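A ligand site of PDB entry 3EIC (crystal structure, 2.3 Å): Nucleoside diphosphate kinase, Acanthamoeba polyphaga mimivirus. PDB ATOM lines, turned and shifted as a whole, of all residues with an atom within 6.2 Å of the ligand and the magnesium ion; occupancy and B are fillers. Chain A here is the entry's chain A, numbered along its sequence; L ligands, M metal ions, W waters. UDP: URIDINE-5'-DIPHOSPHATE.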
ATOM      1  N   LYS A  14      16.588  23.809 -22.907  1.00  0.00           N
ATOM      2  CA  LYS A  14      17.829  23.587 -22.172  1.00  0.00           C
ATOM      3  C   LYS A  14      17.673  23.681 -20.642  1.00  0.00           C
ATOM      4  O   LYS A  14      16.659  24.206 -20.151  1.00  0.00           O
ATOM      5  CB  LYS A  14      18.932  24.519 -22.723  1.00  0.00           C
ATOM      6  CG  LYS A  14      19.106  24.355 -24.234  1.00  0.00           C
ATOM      7  CD  LYS A  14      20.123  25.332 -24.819  1.00  0.00           C
ATOM      8  CE  LYS A  14      20.588  24.906 -26.195  1.00  0.00           C
ATOM      9  NZ  LYS A  14      21.727  25.790 -26.660  1.00  0.00           N
ATOM     10  N   TYR A  55      25.556  17.724 -30.673  1.00  0.00           N
ATOM     11  CA  TYR A  55      26.515  18.792 -30.953  1.00  0.00           C
ATOM     12  C   TYR A  55      27.804  18.340 -31.665  1.00  0.00           C
ATOM     13  O   TYR A  55      28.813  19.030 -31.595  1.00  0.00           O
ATOM     14  CB  TYR A  55      26.837  19.587 -29.674  1.00  0.00           C
ATOM     15  CG  TYR A  55      25.693  20.492 -29.240  1.00  0.00           C
ATOM     16  CD1 TYR A  55      25.014  20.275 -28.040  1.00  0.00           C
ATOM     17  CD2 TYR A  55      25.272  21.564 -30.049  1.00  0.00           C
ATOM     18  CE1 TYR A  55      23.961  21.102 -27.642  1.00  0.00           C
ATOM     19  CE2 TYR A  55      24.212  22.395 -29.656  1.00  0.00           C
ATOM     20  CZ  TYR A  55      23.558  22.152 -28.454  1.00  0.00           C
ATOM     21  OH  TYR A  55      22.515  22.962 -28.065  1.00  0.00           O
ATOM     22  N   HIS A  58      30.279  20.377 -33.565  1.00  0.00           N
ATOM     23  CA  HIS A  58      30.996  21.317 -32.710  1.00  0.00           C
ATOM     24  C   HIS A  58      32.158  20.681 -31.959  1.00  0.00           C
ATOM     25  O   HIS A  58      32.820  21.374 -31.160  1.00  0.00           O
ATOM     26  CB  HIS A  58      30.024  21.925 -31.684  1.00  0.00           C
ATOM     27  CG  HIS A  58      28.903  22.710 -32.293  1.00  0.00           C
ATOM     28  ND1 HIS A  58      28.950  24.071 -32.436  1.00  0.00           N
ATOM     29  CD2 HIS A  58      27.708  22.308 -32.787  1.00  0.00           C
ATOM     30  CE1 HIS A  58      27.835  24.489 -33.007  1.00  0.00           C
ATOM     31  NE2 HIS A  58      27.069  23.442 -33.229  1.00  0.00           N
ATOM     32  N   TYR A  63      34.470  25.618 -26.785  1.00  0.00           N
ATOM     33  CA  TYR A  63      33.275  25.592 -25.917  1.00  0.00           C
ATOM     34  C   TYR A  63      32.609  24.215 -25.848  1.00  0.00           C
ATOM     35  O   TYR A  63      31.743  24.009 -24.998  1.00  0.00           O
ATOM     36  CB  TYR A  63      32.247  26.648 -26.357  1.00  0.00           C
ATOM     37  CG  TYR A  63      31.744  26.469 -27.777  1.00  0.00           C
ATOM     38  CD1 TYR A  63      30.794  25.496 -28.079  1.00  0.00           C
ATOM     39  CD2 TYR A  63      32.225  27.270 -28.807  1.00  0.00           C
ATOM     40  CE1 TYR A  63      30.346  25.324 -29.365  1.00  0.00           C
ATOM     41  CE2 TYR A  63      31.776  27.108 -30.103  1.00  0.00           C
ATOM     42  CZ  TYR A  63      30.840  26.132 -30.371  1.00  0.00           C
ATOM     43  OH  TYR A  63      30.394  25.953 -31.664  1.00  0.00           O
ATOM     44  N   ASP A  66      32.511  22.446 -22.146  1.00  0.00           N
ATOM     45  CA  ASP A  66      31.716  23.258 -21.219  1.00  0.00           C
ATOM     46  C   ASP A  66      30.223  23.204 -21.544  1.00  0.00           C
ATOM     47  O   ASP A  66      29.382  23.250 -20.650  1.00  0.00           O
ATOM     48  CB  ASP A  66      32.174  24.730 -21.220  1.00  0.00           C
ATOM     49  CG  ASP A  66      33.641  24.908 -20.824  1.00  0.00           C
ATOM     50  OD1 ASP A  66      34.052  24.352 -19.770  1.00  0.00           O
ATOM     51  OD2 ASP A  66      34.384  25.624 -21.573  1.00  0.00           O
ATOM     52  N   ASN A  67      29.907  23.102 -22.823  1.00  0.00           N
ATOM     53  CA  ASN A  67      28.518  23.117 -23.234  1.00  0.00           C
ATOM     54  C   ASN A  67      27.805  21.806 -22.933  1.00  0.00           C
ATOM     55  O   ASN A  67      26.684  21.823 -22.393  1.00  0.00           O
ATOM     56  CB  ASN A  67      28.385  23.504 -24.706  1.00  0.00           C
ATOM     57  CG  ASN A  67      26.952  23.714 -25.125  1.00  0.00           C
ATOM     58  OD1 ASN A  67      26.522  23.237 -26.173  1.00  0.00           O
ATOM     59  ND2 ASN A  67      26.188  24.420 -24.300  1.00  0.00           N
ATOM     60  N   PHE A  70      27.065  21.729 -19.254  1.00  0.00           N
ATOM     61  CA  PHE A  70      25.853  22.479 -19.021  1.00  0.00           C
ATOM     62  C   PHE A  70      24.629  21.664 -19.478  1.00  0.00           C
ATOM     63  O   PHE A  70      23.643  21.542 -18.738  1.00  0.00           O
ATOM     64  CB  PHE A  70      25.950  23.853 -19.711  1.00  0.00           C
ATOM     65  CG  PHE A  70      24.625  24.513 -19.972  1.00  0.00           C
ATOM     66  CD1 PHE A  70      24.162  24.670 -21.271  1.00  0.00           C
ATOM     67  CD2 PHE A  70      23.836  24.960 -18.907  1.00  0.00           C
ATOM     68  CE1 PHE A  70      22.924  25.279 -21.523  1.00  0.00           C
ATOM     69  CE2 PHE A  70      22.600  25.553 -19.156  1.00  0.00           C
ATOM     70  CZ  PHE A  70      22.151  25.714 -20.472  1.00  0.00           C
ATOM     71  N   MET A  71      24.715  21.048 -20.658  1.00  0.00           N
ATOM     72  CA  MET A  71      23.597  20.285 -21.197  1.00  0.00           C
ATOM     73  C   MET A  71      23.201  19.084 -20.345  1.00  0.00           C
ATOM     74  O   MET A  71      22.064  18.573 -20.464  1.00  0.00           O
ATOM     75  CB  MET A  71      23.841  19.903 -22.657  1.00  0.00           C
ATOM     76  CG  MET A  71      23.750  21.070 -23.657  1.00  0.00           C
ATOM     77  SD  MET A  71      22.170  21.979 -23.594  1.00  0.00           S
ATOM     78  CE  MET A  71      21.083  20.843 -24.481  1.00  0.00           C
ATOM     79  N   ARG A  91      13.241  28.509 -35.931  1.00  0.00           N
ATOM     80  CA  ARG A  91      14.596  29.041 -35.812  1.00  0.00           C
ATOM     81  C   ARG A  91      14.592  30.536 -35.592  1.00  0.00           C
ATOM     82  O   ARG A  91      15.356  31.037 -34.791  1.00  0.00           O
ATOM     83  CB  ARG A  91      15.414  28.737 -37.067  1.00  0.00           C
ATOM     84  CG  ARG A  91      16.678  27.960 -36.780  1.00  0.00           C
ATOM     85  CD  ARG A  91      17.869  28.860 -36.580  1.00  0.00           C
ATOM     86  NE  ARG A  91      18.776  28.292 -35.577  1.00  0.00           N
ATOM     87  CZ  ARG A  91      20.086  28.515 -35.534  1.00  0.00           C
ATOM     88  NH1 ARG A  91      20.675  29.267 -36.451  1.00  0.00           N
ATOM     89  NH2 ARG A  91      20.799  27.958 -34.561  1.00  0.00           N
ATOM     90  N   GLN A  94      13.502  31.344 -32.131  1.00  0.00           N
ATOM     91  CA  GLN A  94      14.636  31.159 -31.231  1.00  0.00           C
ATOM     92  C   GLN A  94      15.502  32.407 -31.264  1.00  0.00           C
ATOM     93  O   GLN A  94      15.834  32.962 -30.227  1.00  0.00           O
ATOM     94  CB  GLN A  94      15.448  29.903 -31.613  1.00  0.00           C
ATOM     95  CG  GLN A  94      16.838  29.828 -30.977  1.00  0.00           C
ATOM     96  CD  GLN A  94      17.859  29.079 -31.830  1.00  0.00           C
ATOM     97  OE1 GLN A  94      17.865  27.845 -31.887  1.00  0.00           O
ATOM     98  NE2 GLN A  94      18.749  29.817 -32.491  1.00  0.00           N
ATOM     99  N   GLY A  95      15.834  32.875 -32.465  1.00  0.00           N
ATOM    100  CA  GLY A  95      16.619  34.095 -32.627  1.00  0.00           C
ATOM    101  C   GLY A  95      17.949  34.038 -31.889  1.00  0.00           C
ATOM    102  O   GLY A  95      18.572  32.969 -31.782  1.00  0.00           O
ATOM    103  N   ASN A  96      18.377  35.187 -31.362  1.00  0.00           N
ATOM    104  CA  ASN A  96      19.660  35.289 -30.653  1.00  0.00           C
ATOM    105  C   ASN A  96      19.552  36.330 -29.561  1.00  0.00           C
ATOM    106  O   ASN A  96      18.570  37.077 -29.519  1.00  0.00           O
ATOM    107  CB  ASN A  96      20.810  35.605 -31.615  1.00  0.00           C
ATOM    108  CG  ASN A  96      20.605  36.899 -32.374  1.00  0.00           C
ATOM    109  OD1 ASN A  96      20.366  37.967 -31.800  1.00  0.00           O
ATOM    110  ND2 ASN A  96      20.716  36.819 -33.692  1.00  0.00           N
ATOM    111  N   ARG A 104      15.398  33.993 -27.405  1.00  0.00           N
ATOM    112  CA  ARG A 104      16.694  34.344 -26.826  1.00  0.00           C
ATOM    113  C   ARG A 104      16.811  35.844 -26.649  1.00  0.00           C
ATOM    114  O   ARG A 104      17.386  36.311 -25.669  1.00  0.00           O
ATOM    115  CB  ARG A 104      17.843  33.831 -27.702  1.00  0.00           C
ATOM    116  CG  ARG A 104      17.995  32.343 -27.656  1.00  0.00           C
ATOM    117  CD  ARG A 104      19.151  31.924 -28.513  1.00  0.00           C
ATOM    118  NE  ARG A 104      19.260  30.483 -28.640  1.00  0.00           N
ATOM    119  CZ  ARG A 104      20.252  29.870 -29.276  1.00  0.00           C
ATOM    120  NH1 ARG A 104      21.241  30.570 -29.822  1.00  0.00           N
ATOM    121  NH2 ARG A 104      20.251  28.544 -29.368  1.00  0.00           N
ATOM    122  N   ILE A 111      26.182  33.443 -23.970  1.00  0.00           N
ATOM    123  CA  ILE A 111      26.611  32.647 -25.151  1.00  0.00           C
ATOM    124  C   ILE A 111      26.370  31.147 -25.012  1.00  0.00           C
ATOM    125  O   ILE A 111      26.284  30.437 -26.004  1.00  0.00           O
ATOM    126  CB  ILE A 111      28.138  32.769 -25.464  1.00  0.00           C
ATOM    127  CG1 ILE A 111      28.975  32.741 -24.165  1.00  0.00           C
ATOM    128  CG2 ILE A 111      28.410  33.946 -26.399  1.00  0.00           C
ATOM    129  CD1 ILE A 111      30.510  32.814 -24.350  1.00  0.00           C
ATOM    130  N   ARG A 112      26.298  30.659 -23.789  1.00  0.00           N
ATOM    131  CA  ARG A 112      26.133  29.225 -23.561  1.00  0.00           C
ATOM    132  C   ARG A 112      24.720  28.913 -23.072  1.00  0.00           C
ATOM    133  O   ARG A 112      24.003  28.111 -23.693  1.00  0.00           O
ATOM    134  CB  ARG A 112      27.193  28.735 -22.556  1.00  0.00           C
ATOM    135  CG  ARG A 112      27.248  27.220 -22.307  1.00  0.00           C
ATOM    136  CD  ARG A 112      28.258  26.911 -21.195  1.00  0.00           C
ATOM    137  NE  ARG A 112      27.606  26.792 -19.889  1.00  0.00           N
ATOM    138  CZ  ARG A 112      28.174  27.068 -18.708  1.00  0.00           C
ATOM    139  NH1 ARG A 112      29.420  27.519 -18.639  1.00  0.00           N
ATOM    140  NH2 ARG A 112      27.473  26.898 -17.577  1.00  0.00           N
ATOM    141  N   GLU A 113      24.315  29.557 -21.976  1.00  0.00           N
ATOM    142  CA  GLU A 113      23.010  29.333 -21.372  1.00  0.00           C
ATOM    143  C   GLU A 113      21.964  30.189 -22.101  1.00  0.00           C
ATOM    144  O   GLU A 113      21.709  31.363 -21.774  1.00  0.00           O
ATOM    145  CB  GLU A 113      23.055  29.606 -19.879  1.00  0.00           C
ATOM    146  CG  GLU A 113      24.160  28.828 -19.164  1.00  0.00           C
ATOM    147  CD  GLU A 113      24.079  28.894 -17.650  1.00  0.00           C
ATOM    148  OE1 GLU A 113      23.312  29.725 -17.134  1.00  0.00           O
ATOM    149  OE2 GLU A 113      24.779  28.103 -16.960  1.00  0.00           O
ATOM    150  N   ASN A 114      21.360  29.584 -23.116  1.00  0.00           N
ATOM    151  CA  ASN A 114      20.504  30.333 -24.008  1.00  0.00           C
ATOM    152  C   ASN A 114      19.158  29.652 -24.246  1.00  0.00           C
ATOM    153  O   ASN A 114      18.541  29.821 -25.291  1.00  0.00           O
ATOM    154  CB  ASN A 114      21.246  30.699 -25.312  1.00  0.00           C
ATOM    155  CG  ASN A 114      21.795  29.485 -26.045  1.00  0.00           C
ATOM    156  OD1 ASN A 114      21.453  28.319 -25.748  1.00  0.00           O
ATOM    157  ND2 ASN A 114      22.653  29.743 -27.038  1.00  0.00           N
ATOM    158  N   ILE A 116      17.190  27.556 -25.394  1.00  0.00           N
ATOM    159  CA  ILE A 116      16.584  26.738 -26.462  1.00  0.00           C
ATOM    160  C   ILE A 116      17.507  26.446 -27.653  1.00  0.00           C
ATOM    161  O   ILE A 116      18.291  27.306 -28.051  1.00  0.00           O
ATOM    162  CB  ILE A 116      15.288  27.405 -26.990  1.00  0.00           C
ATOM    163  CG1 ILE A 116      14.683  26.628 -28.145  1.00  0.00           C
ATOM    164  CG2 ILE A 116      15.539  28.888 -27.388  1.00  0.00           C
ATOM    165  CD1 ILE A 116      13.364  27.209 -28.644  1.00  0.00           C
ATOM    166  N   HIS A 117      17.412  25.228 -28.183  1.00  0.00           N
ATOM    167  CA  HIS A 117      17.954  24.856 -29.502  1.00  0.00           C
ATOM    168  C   HIS A 117      16.834  24.535 -30.493  1.00  0.00           C
ATOM    169  O   HIS A 117      15.868  23.835 -30.135  1.00  0.00           O
ATOM    170  CB  HIS A 117      18.854  23.620 -29.405  1.00  0.00           C
ATOM    171  CG  HIS A 117      19.137  22.984 -30.737  1.00  0.00           C
ATOM    172  ND1 HIS A 117      20.282  23.232 -31.451  1.00  0.00           N
ATOM    173  CD2 HIS A 117      18.392  22.134 -31.486  1.00  0.00           C
ATOM    174  CE1 HIS A 117      20.248  22.558 -32.591  1.00  0.00           C
ATOM    175  NE2 HIS A 117      19.106  21.895 -32.638  1.00  0.00           N
ATOM    176  N   ALA A 118      16.964  25.025 -31.723  1.00  0.00           N
ATOM    177  CA  ALA A 118      16.126  24.598 -32.862  1.00  0.00           C
ATOM    178  C   ALA A 118      17.028  24.158 -34.032  1.00  0.00           C
ATOM    179  O   ALA A 118      18.095  24.712 -34.220  1.00  0.00           O
ATOM    180  CB  ALA A 118      15.244  25.728 -33.311  1.00  0.00           C
ATOM    181  N   ASP A 120      18.585  23.996 -37.629  1.00  0.00           N
ATOM    182  CA  ASP A 120      18.774  25.103 -38.549  1.00  0.00           C
ATOM    183  C   ASP A 120      18.649  24.747 -40.040  1.00  0.00           C
ATOM    184  O   ASP A 120      18.786  25.638 -40.901  1.00  0.00           O
ATOM    185  CB  ASP A 120      20.102  25.811 -38.284  1.00  0.00           C
ATOM    186  CG  ASP A 120      21.307  24.970 -38.628  1.00  0.00           C
ATOM    187  OD1 ASP A 120      21.116  23.812 -39.090  1.00  0.00           O
ATOM    188  OD2 ASP A 120      22.438  25.466 -38.434  1.00  0.00           O
HETATM  189  N1  UDP L   1      27.950  27.716 -27.345  1.00  0.00           N
HETATM  190  C2  UDP L   1      28.750  28.018 -26.240  1.00  0.00           C
HETATM  191  N3  UDP L   1      29.766  28.941 -26.342  1.00  0.00           N
HETATM  192  C4  UDP L   1      29.994  29.581 -27.553  1.00  0.00           C
HETATM  193  C5  UDP L   1      29.178  29.285 -28.651  1.00  0.00           C
HETATM  194  C6  UDP L   1      28.274  28.237 -28.574  1.00  0.00           C
HETATM  195  O2  UDP L   1      28.584  27.447 -25.166  1.00  0.00           O
HETATM  196  O4  UDP L   1      30.896  30.410 -27.648  1.00  0.00           O
HETATM  197  C1' UDP L   1      26.836  26.727 -27.204  1.00  0.00           C
HETATM  198  C2' UDP L   1      25.497  27.467 -27.156  1.00  0.00           C
HETATM  199  O2' UDP L   1      24.659  26.897 -26.182  1.00  0.00           O
HETATM  200  C3' UDP L   1      24.912  27.261 -28.532  1.00  0.00           C
HETATM  201  C4' UDP L   1      25.508  25.921 -28.962  1.00  0.00           C
HETATM  202  O4' UDP L   1      26.778  25.836 -28.308  1.00  0.00           O
HETATM  203  O3' UDP L   1      23.504  27.251 -28.509  1.00  0.00           O
HETATM  204  C5' UDP L   1      25.741  25.839 -30.463  1.00  0.00           C
HETATM  205  O5' UDP L   1      26.499  26.961 -30.849  1.00  0.00           O
HETATM  206  PA  UDP L   1      25.984  27.911 -32.028  1.00  0.00           P
HETATM  207  O1A UDP L   1      25.693  27.094 -33.235  1.00  0.00           O
HETATM  208  O2A UDP L   1      26.977  28.986 -32.296  1.00  0.00           O
HETATM  209  O3A UDP L   1      24.636  28.654 -31.503  1.00  0.00           O
HETATM  210  PB  UDP L   1      23.101  28.362 -31.935  1.00  0.00           P
HETATM  211  O1B UDP L   1      22.380  29.645 -31.860  1.00  0.00           O
HETATM  212  O2B UDP L   1      22.544  27.365 -30.989  1.00  0.00           O
HETATM  213  O3B UDP L   1      22.963  27.860 -33.318  1.00  0.00           O
HETATM  214 MG    MG M   1      24.262  26.806 -34.607  1.00  0.00          MG
HETATM  215  O   HOH W   1      23.704  24.544 -25.319  1.00  0.00           O
HETATM  216  O   HOH W   2      22.002  25.112 -29.781  1.00  0.00           O
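NH2 of Arg 91 lies within salt-bridge range of O1B of the ligand. NH1 of Arg 104 is in salt-bridge range of O1B of the ligand (2.5 Å). The backbone carbonyl oxygen of Arg 112 lies within hydrogen-bond range of an oxygen (O2') of the ligand (2.8 Å). The side-chain amino group (NZ) of Lys 14 is in hydrogen-bond range of an oxygen (O3') of the ligand. ND2 of Asn 114 lies within hydrogen-bond range of O3' of the ligand, 3.0 Å away. The side-chain amide oxygen (OD1) of Asn 67 lies close to an oxygen (O4') of the ligand (3.4 Å).
NE2 of Gln 94 lies close to NE of Arg 91, 3.4 Å away. The backbone NH (N) of Arg 104 sits at hydrogen-bond distance from the backbone carbonyl oxygen (O) of Gln 94 (3.0 Å). The backbone carbonyl oxygen (O) of Ile 116 is in hydrogen-bond range of the guanidinium group (NH2) of Arg 104, 2.7 Å away. O of Arg 112 sits close to OD1 of Asn 114 (3.3 Å). The side-chain amino group (NZ) of Lys 14 sits at hydrogen-bond distance from the side-chain amide oxygen (OD1) of Asn 114 (2.7 Å). The side-chain hydroxyl (OH) of Tyr 55 lies within hydrogen-bond range of the side-chain amino group (NZ) of Lys 14 (3.3 Å). OH of Tyr 63 is in hydrogen-bond range of ND1 of His 58 (2.5 Å). N of Ala 118 lies within hydrogen-bond range of OE1 of Gln 94, 3.0 Å away.
O of Ile 111 lies close to N1 of the ligand, at 3.5 Å. Merely in contact with the ligand: Tyr 55 (3.8 Å), His 58 (3.4 Å), Tyr 63 (3.4 Å) and Gln 94 (3.7 Å).
Arg 91 touches the magnesium ion. The nearest printed residue that does not touch the magnesium ion is Asp 120 (4.4 Å).
The magnesium ion is bound by an oxygen (O1A) of the ligand and an oxygen (O3B) of the ligand.
Water W2 lies within hydrogen-bond range of O2B of the ligand (2.6 Å), OH of Tyr 55 (2.8 Å), ND1 of His 117 (3.0 Å) and NZ of Lys 14 (3.2 Å). Water W1 lies within hydrogen-bond range of O2' of the ligand (2.7 Å), ND2 of Asn 67 (2.7 Å), NZ of Lys 14 (2.7 Å), OH of Tyr 55 (3.4 Å) and SD of Met 71 (3.5 Å).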
